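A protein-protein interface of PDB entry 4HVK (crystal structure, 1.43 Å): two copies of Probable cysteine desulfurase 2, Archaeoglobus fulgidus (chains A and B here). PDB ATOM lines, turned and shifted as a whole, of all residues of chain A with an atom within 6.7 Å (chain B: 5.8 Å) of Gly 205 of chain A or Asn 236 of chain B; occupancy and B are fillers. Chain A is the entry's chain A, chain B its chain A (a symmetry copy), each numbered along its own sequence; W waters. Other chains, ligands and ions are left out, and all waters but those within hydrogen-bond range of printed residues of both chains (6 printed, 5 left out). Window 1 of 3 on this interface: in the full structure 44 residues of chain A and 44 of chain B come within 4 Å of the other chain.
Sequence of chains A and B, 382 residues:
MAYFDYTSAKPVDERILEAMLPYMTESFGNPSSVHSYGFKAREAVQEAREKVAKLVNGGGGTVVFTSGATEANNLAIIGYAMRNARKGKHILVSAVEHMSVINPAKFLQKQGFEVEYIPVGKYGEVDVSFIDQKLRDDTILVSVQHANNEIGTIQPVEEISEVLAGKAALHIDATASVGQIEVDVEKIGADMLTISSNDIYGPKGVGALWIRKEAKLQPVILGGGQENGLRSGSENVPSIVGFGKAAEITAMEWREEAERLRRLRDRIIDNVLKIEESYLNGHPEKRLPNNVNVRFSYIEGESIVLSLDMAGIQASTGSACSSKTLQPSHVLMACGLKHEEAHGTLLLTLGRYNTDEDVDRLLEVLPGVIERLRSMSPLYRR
ND2 of Asn 236 of chain B is in hydrogen-bond range of O of Lys 204 of chain A (3.4 Å). The side-chain hydroxyl of Ser 67 of chain B is in hydrogen-bond range of the guanidinium group of Arg 231 of chain A (3.5 Å).
The backbone carbonyl oxygen (O) of Ser 67 of chain B is in hydrogen-bond range of the backbone NH (N) of Val 206 of chain B (3.3 Å). OG of Ser 239 of chain A is in hydrogen-bond range of ND2 of Asn 236 of chain A (2.8 Å). O of Ser 67 of chain A is in hydrogen-bond range of N of Val 206 of chain A (3.3 Å). OG of Ser 239 of chain B lies within hydrogen-bond range of ND2 of Asn 236 of chain B (2.8 Å).
CB of Ser 67 of chain A touches CB of Ser 67 of chain B, at 3.7 Å. O of Glu 235 of chain B touches CD of Lys 204 of chain A, at 3.8 Å. ND2 of Asn 236 of chain B touches CA of Gly 205 of chain A, 3.4 Å away. ND2 of Asn 236 of chain A touches CA of Gly 205 of chain B, 3.4 Å away.
Of chain B, only Asn 236 (3.4 Å) comes within 4 Å of Gly 205 of chain A. Printed residues of chain A within 4 Å of Ser 67 of chain B: Ser 67 and Arg 231. Of the printed residues of chain B, Asn 236 of chain A touches Gly 205 (3.4 Å). Thr 66 of chain A touches none of the printed residues of chain B. The nearest residue of chain A that does not touch Asn 236 of chain B is Ser 239 of chain A (5.4 Å).
Of the 13 printed residues of chain A, 5 touch a printed residue of chain B. Among the printed residues, no Asp or Glu carboxylate lies within 4 Å of a Lys or Arg side-chain nitrogen of the other chain.
Ser 67 of chain A touches its own counterpart, Ser 67 of chain B. Gly 205 of chain A touches Asn 236 of chain B, and with the chains exchanged Asn 236 of chain A touches Gly 205 of chain B. 5 positions are printed for both chains. Of the 6 pairs that touch across the chains among the printed residues, 3 have their exchanged pair printed and touching as well.
Water W6 lies within hydrogen-bond range of O of Lys 204 of chain A (2.5 Å), OG of Ser 239 of chain A (2.6 Å), ND2 of Asn 236 of chain B (2.8 Å) and ND2 of Asn 236 of chain A (3.5 Å). Water W4 lies within hydrogen-bond range of the side-chain hydroxyl of Ser 239 of chain B (2.6 Å), the side-chain amide nitrogen of Asn 236 of chain A (2.8 Å) and the side-chain amide nitrogen of Asn 236 of chain B (3.5 Å). Water W3 bridges OD1 of Asn 236 of chain B and O of Lys 204 of chain A. Water W5 lies within hydrogen-bond range of the backbone carbonyl oxygen of Glu 235 of chain B (2.8 Å) and the side-chain amino group of Lys 204 of chain A (2.9 Å). Water W1 bridges the backbone NH (N) of Gly 205 of chain A (3.0 Å) and the backbone carbonyl oxygen (O) of Ser 234 of chain B (3.0 Å). Water W2 lies within hydrogen-bond range of OG of Ser 67 of chain B and NH2 of Arg 231 of chain A.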
ATOM      1  N   THR A  66       4.541 -14.514  12.733  1.00  0.00           N
ATOM      2  CA  THR A  66       4.291 -15.699  11.964  1.00  0.00           C
ATOM      3  C   THR A  66       4.407 -16.921  12.845  1.00  0.00           C
ATOM      4  O   THR A  66       4.687 -16.813  14.071  1.00  0.00           O
ATOM      5  CB  THR A  66       5.349 -15.844  10.865  1.00  0.00           C
ATOM      6  OG1 THR A  66       6.623 -16.068  11.478  1.00  0.00           O
ATOM      7  CG2 THR A  66       5.338 -14.601   9.901  1.00  0.00           C
ATOM      8  N   SER A  67       4.248 -18.104  12.275  1.00  0.00           N
ATOM      9  CA  SER A  67       4.434 -19.359  12.977  1.00  0.00           C
ATOM     10  C   SER A  67       5.896 -19.811  13.044  1.00  0.00           C
ATOM     11  O   SER A  67       6.168 -20.924  13.503  1.00  0.00           O
ATOM     12  CB  SER A  67       3.606 -20.463  12.337  1.00  0.00           C
ATOM     13  OG  SER A  67       4.132 -20.692  10.984  1.00  0.00           O
ATOM     14  N   GLY A  68       6.830 -18.960  12.625  1.00  0.00           N
ATOM     15  CA  GLY A  68       8.230 -19.305  12.636  1.00  0.00           C
ATOM     16  C   GLY A  68       8.999 -18.724  11.490  1.00  0.00           C
ATOM     17  O   GLY A  68       8.419 -18.040  10.599  1.00  0.00           O
ATOM     18  N   SER A 197      11.911 -17.173  16.828  1.00  0.00           N
ATOM     19  CA  SER A 197      11.780 -17.156  18.276  1.00  0.00           C
ATOM     20  C   SER A 197      12.637 -18.224  18.927  1.00  0.00           C
ATOM     21  O   SER A 197      13.380 -17.944  19.912  1.00  0.00           O
ATOM     22  CB  SER A 197      10.308 -17.361  18.654  1.00  0.00           C
ATOM     23  OG  SER A 197      10.167 -17.593  20.033  1.00  0.00           O
ATOM     24  N   ASN A 198      12.555 -19.496  18.514  1.00  0.00           N
ATOM     25  CA  ASN A 198      13.276 -20.492  19.259  1.00  0.00           C
ATOM     26  C   ASN A 198      14.786 -20.325  19.123  1.00  0.00           C
ATOM     27  O   ASN A 198      15.533 -20.752  19.988  1.00  0.00           O
ATOM     28  CB  ASN A 198      12.810 -21.919  18.842  1.00  0.00           C
ATOM     29  CG  ASN A 198      13.439 -23.002  19.700  1.00  0.00           C
ATOM     30  OD1 ASN A 198      14.117 -23.890  19.164  1.00  0.00           O
ATOM     31  ND2 ASN A 198      13.177 -22.987  21.014  1.00  0.00           N
ATOM     32  N   PRO A 203       9.776 -19.655  22.555  1.00  0.00           N
ATOM     33  CA  PRO A 203       9.041 -20.840  22.154  1.00  0.00           C
ATOM     34  C   PRO A 203       9.183 -21.101  20.680  1.00  0.00           C
ATOM     35  O   PRO A 203       9.268 -20.178  19.823  1.00  0.00           O
ATOM     36  CB  PRO A 203       7.587 -20.498  22.526  1.00  0.00           C
ATOM     37  CG  PRO A 203       7.563 -19.094  22.611  1.00  0.00           C
ATOM     38  CD  PRO A 203       8.878 -18.578  22.964  1.00  0.00           C
ATOM     39  N   LYS A 204       9.095 -22.398  20.294  1.00  0.00           N
ATOM     40  CA  LYS A 204       8.922 -22.829  18.924  1.00  0.00           C
ATOM     41  C   LYS A 204       7.546 -22.390  18.413  1.00  0.00           C
ATOM     42  O   LYS A 204       6.664 -22.059  19.222  1.00  0.00           O
ATOM     43  CB  LYS A 204       9.047 -24.328  18.844  1.00  0.00           C
ATOM     44  CG  LYS A 204      10.396 -24.860  19.210  1.00  0.00           C
ATOM     45  CD  LYS A 204      10.449 -26.404  19.256  1.00  0.00           C
ATOM     46  CE  LYS A 204      11.832 -26.949  19.593  1.00  0.00           C
ATOM     47  NZ  LYS A 204      11.821 -28.429  19.649  1.00  0.00           N
ATOM     48  N   GLY A 205       7.330 -22.440  17.104  1.00  0.00           N
ATOM     49  CA  GLY A 205       6.014 -22.170  16.587  1.00  0.00           C
ATOM     50  C   GLY A 205       5.593 -20.727  16.457  1.00  0.00           C
ATOM     51  O   GLY A 205       4.445 -20.436  16.229  1.00  0.00           O
ATOM     52  N   VAL A 206       6.557 -19.844  16.580  1.00  0.00           N
ATOM     53  CA  VAL A 206       6.374 -18.398  16.347  1.00  0.00           C
ATOM     54  C   VAL A 206       7.698 -17.809  15.836  1.00  0.00           C
ATOM     55  O   VAL A 206       8.806 -18.367  16.034  1.00  0.00           O
ATOM     56  CB  VAL A 206       5.898 -17.713  17.651  1.00  0.00           C
ATOM     57  CG1 VAL A 206       6.944 -17.796  18.782  1.00  0.00           C
ATOM     58  CG2 VAL A 206       5.460 -16.253  17.442  1.00  0.00           C
ATOM     59  N   GLY A 207       7.517 -16.720  15.117  1.00  0.00           N
ATOM     60  CA  GLY A 207       8.636 -15.990  14.551  1.00  0.00           C
ATOM     61  C   GLY A 207       8.077 -14.699  14.009  1.00  0.00           C
ATOM     62  O   GLY A 207       6.975 -14.317  14.293  1.00  0.00           O
ATOM     63  N   ARG A 231      -1.182 -11.370   7.818  1.00  0.00           N
ATOM     64  CA  ARG A 231      -1.056 -12.736   8.340  1.00  0.00           C
ATOM     65  C   ARG A 231      -2.216 -13.024   9.244  1.00  0.00           C
ATOM     66  O   ARG A 231      -2.224 -12.663  10.422  1.00  0.00           O
ATOM     67  CB  ARG A 231       0.318 -12.901   8.987  1.00  0.00           C
ATOM     68  CG  ARG A 231       0.715 -14.346   9.252  1.00  0.00           C
ATOM     69  CD  ARG A 231       0.213 -14.847  10.593  1.00  0.00           C
ATOM     70  NE  ARG A 231       0.626 -16.223  10.809  1.00  0.00           N
ATOM     71  CZ  ARG A 231       0.246 -16.949  11.840  1.00  0.00           C
ATOM     72  NH1 ARG A 231      -0.632 -16.440  12.693  1.00  0.00           N
ATOM     73  NH2 ARG A 231       0.704 -18.158  11.997  1.00  0.00           N
ATOM     74  N   ASN A 236      -1.519 -16.048  18.615  1.00  0.00           N
ATOM     75  CA  ASN A 236      -1.024 -16.989  19.621  1.00  0.00           C
ATOM     76  C   ASN A 236      -0.326 -16.170  20.710  1.00  0.00           C
ATOM     77  O   ASN A 236       0.885 -16.022  20.738  1.00  0.00           O
ATOM     78  CB  ASN A 236      -0.067 -17.976  19.013  1.00  0.00           C
ATOM     79  CG  ASN A 236       0.495 -18.963  19.980  1.00  0.00           C
ATOM     80  OD1 ASN A 236       0.238 -18.893  21.236  1.00  0.00           O
ATOM     81  ND2 ASN A 236       1.270 -19.865  19.461  1.00  0.00           N
ATOM     82  N   SER A 239       2.737 -17.499  22.867  1.00  0.00           N
ATOM     83  CA  SER A 239       3.989 -17.642  22.172  1.00  0.00           C
ATOM     84  C   SER A 239       4.589 -16.266  21.792  1.00  0.00           C
ATOM     85  O   SER A 239       5.810 -16.083  21.831  1.00  0.00           O
ATOM     86  CB  SER A 239       3.794 -18.465  20.913  1.00  0.00           C
ATOM     87  OG  SER A 239       3.440 -19.794  21.232  1.00  0.00           O
ATOM     88  N   SER B  67      -0.461 -24.197  12.003  1.00  0.00           N
ATOM     89  CA  SER B  67      -0.433 -23.184  13.041  1.00  0.00           C
ATOM     90  C   SER B  67      -1.821 -22.815  13.572  1.00  0.00           C
ATOM     91  O   SER B  67      -1.941 -21.877  14.364  1.00  0.00           O
ATOM     92  CB  SER B  67       0.256 -21.922  12.544  1.00  0.00           C
ATOM     93  OG  SER B  67      -0.568 -21.354  11.469  1.00  0.00           O
ATOM     94  N   GLY B 205      -2.164 -21.427  18.410  1.00  0.00           N
ATOM     95  CA  GLY B 205      -1.018 -21.504  17.542  1.00  0.00           C
ATOM     96  C   GLY B 205      -0.688 -22.844  16.933  1.00  0.00           C
ATOM     97  O   GLY B 205       0.363 -23.024  16.369  1.00  0.00           O
ATOM     98  N   VAL B 206      -1.624 -23.758  17.038  1.00  0.00           N
ATOM     99  CA  VAL B 206      -1.549 -25.081  16.386  1.00  0.00           C
ATOM    100  C   VAL B 206      -2.975 -25.554  16.065  1.00  0.00           C
ATOM    101  O   VAL B 206      -3.986 -25.107  16.662  1.00  0.00           O
ATOM    102  CB  VAL B 206      -0.801 -26.076  17.306  1.00  0.00           C
ATOM    103  CG1 VAL B 206      -1.545 -26.336  18.632  1.00  0.00           C
ATOM    104  CG2 VAL B 206      -0.473 -27.411  16.614  1.00  0.00           C
ATOM    105  N   SER B 234      10.073 -26.469  11.199  1.00  0.00           N
ATOM    106  CA  SER B 234      10.440 -27.343  12.291  1.00  0.00           C
ATOM    107  C   SER B 234       9.209 -27.505  13.197  1.00  0.00           C
ATOM    108  O   SER B 234       8.530 -26.502  13.529  1.00  0.00           O
ATOM    109  CB  SER B 234      11.612 -26.780  13.096  1.00  0.00           C
ATOM    110  OG  SER B 234      12.778 -26.703  12.287  1.00  0.00           O
ATOM    111  N   GLU B 235       8.962 -28.736  13.634  1.00  0.00           N
ATOM    112  CA  GLU B 235       7.755 -28.983  14.381  1.00  0.00           C
ATOM    113  C   GLU B 235       7.721 -28.283  15.705  1.00  0.00           C
ATOM    114  O   GLU B 235       8.710 -28.317  16.448  1.00  0.00           O
ATOM    115  CB  GLU B 235       7.596 -30.484  14.595  1.00  0.00           C
ATOM    116  CG  GLU B 235       7.355 -31.352  13.379  1.00  0.00           C
ATOM    117  CD  GLU B 235       8.626 -31.830  12.643  1.00  0.00           C
ATOM    118  OE1 GLU B 235       9.710 -31.244  12.859  1.00  0.00           O
ATOM    119  OE2 GLU B 235       8.492 -32.757  11.821  1.00  0.00           O
ATOM    120  N   ASN B 236       6.574 -27.694  15.998  1.00  0.00           N
ATOM    121  CA  ASN B 236       6.364 -27.075  17.309  1.00  0.00           C
ATOM    122  C   ASN B 236       5.916 -28.180  18.270  1.00  0.00           C
ATOM    123  O   ASN B 236       4.742 -28.370  18.543  1.00  0.00           O
ATOM    124  CB  ASN B 236       5.323 -25.993  17.234  1.00  0.00           C
ATOM    125  CG  ASN B 236       5.039 -25.323  18.536  1.00  0.00           C
ATOM    126  OD1 ASN B 236       5.584 -25.720  19.628  1.00  0.00           O
ATOM    127  ND2 ASN B 236       4.193 -24.340  18.479  1.00  0.00           N
ATOM    128  N   VAL B 237       6.899 -28.932  18.767  1.00  0.00           N
ATOM    129  CA  VAL B 237       6.608 -30.156  19.580  1.00  0.00           C
ATOM    130  C   VAL B 237       5.753 -29.852  20.794  1.00  0.00           C
ATOM    131  O   VAL B 237       4.781 -30.577  20.969  1.00  0.00           O
ATOM    132  CB  VAL B 237       7.868 -30.927  19.891  1.00  0.00           C
ATOM    133  CG1 VAL B 237       7.529 -32.199  20.733  1.00  0.00           C
ATOM    134  CG2 VAL B 237       8.668 -31.269  18.631  1.00  0.00           C
ATOM    135  N   PRO B 238       6.048 -28.817  21.604  1.00  0.00           N
ATOM    136  CA  PRO B 238       5.212 -28.621  22.760  1.00  0.00           C
ATOM    137  C   PRO B 238       3.766 -28.380  22.430  1.00  0.00           C
ATOM    138  O   PRO B 238       2.836 -28.907  23.039  1.00  0.00           O
ATOM    139  CB  PRO B 238       5.855 -27.438  23.452  1.00  0.00           C
ATOM    140  CG  PRO B 238       7.293 -27.463  23.006  1.00  0.00           C
ATOM    141  CD  PRO B 238       7.192 -27.855  21.590  1.00  0.00           C
ATOM    142  N   SER B 239       3.498 -27.584  21.368  1.00  0.00           N
ATOM    143  CA  SER B 239       2.122 -27.300  21.054  1.00  0.00           C
ATOM    144  C   SER B 239       1.404 -28.542  20.471  1.00  0.00           C
ATOM    145  O   SER B 239       0.222 -28.769  20.748  1.00  0.00           O
ATOM    146  CB  SER B 239       2.040 -26.163  20.055  1.00  0.00           C
ATOM    147  OG  SER B 239       2.504 -24.957  20.627  1.00  0.00           O
ATOM    148  N   ILE B 240       2.147 -29.278  19.649  1.00  0.00           N
ATOM    149  CA  ILE B 240       1.664 -30.533  19.105  1.00  0.00           C
ATOM    150  C   ILE B 240       1.304 -31.512  20.264  1.00  0.00           C
ATOM    151  O   ILE B 240       0.230 -32.115  20.254  1.00  0.00           O
ATOM    152  CB  ILE B 240       2.614 -31.138  18.093  1.00  0.00           C
ATOM    153  CG1 ILE B 240       2.624 -30.347  16.778  1.00  0.00           C
ATOM    154  CG2 ILE B 240       2.309 -32.646  17.853  1.00  0.00           C
ATOM    155  CD1 ILE B 240       3.817 -30.623  15.848  1.00  0.00           C
ATOM    156  N   VAL B 241       2.207 -31.663  21.231  1.00  0.00           N
ATOM    157  CA  VAL B 241       1.914 -32.523  22.377  1.00  0.00           C
ATOM    158  C   VAL B 241       0.656 -32.065  23.106  1.00  0.00           C
ATOM    159  O   VAL B 241      -0.173 -32.873  23.467  1.00  0.00           O
ATOM    160  CB  VAL B 241       3.123 -32.593  23.273  1.00  0.00           C
ATOM    161  CG1 VAL B 241       2.771 -33.266  24.597  1.00  0.00           C
ATOM    162  CG2 VAL B 241       4.264 -33.370  22.569  1.00  0.00           C
HETATM  163  O   HOH W   1       8.852 -24.004  15.100  1.00  0.00           O
HETATM  164  O   HOH W   2      -2.369 -18.623  10.483  1.00  0.00           O
HETATM  165  O   HOH W   3       5.950 -23.922  21.542  1.00  0.00           O
HETATM  166  O   HOH W   4       1.443 -22.687  19.816  1.00  0.00           O
HETATM  167  O   HOH W   5      11.373 -28.965  16.865  1.00  0.00           O
HETATM  168  O   HOH W   6       4.202 -21.726  19.611  1.00  0.00           O
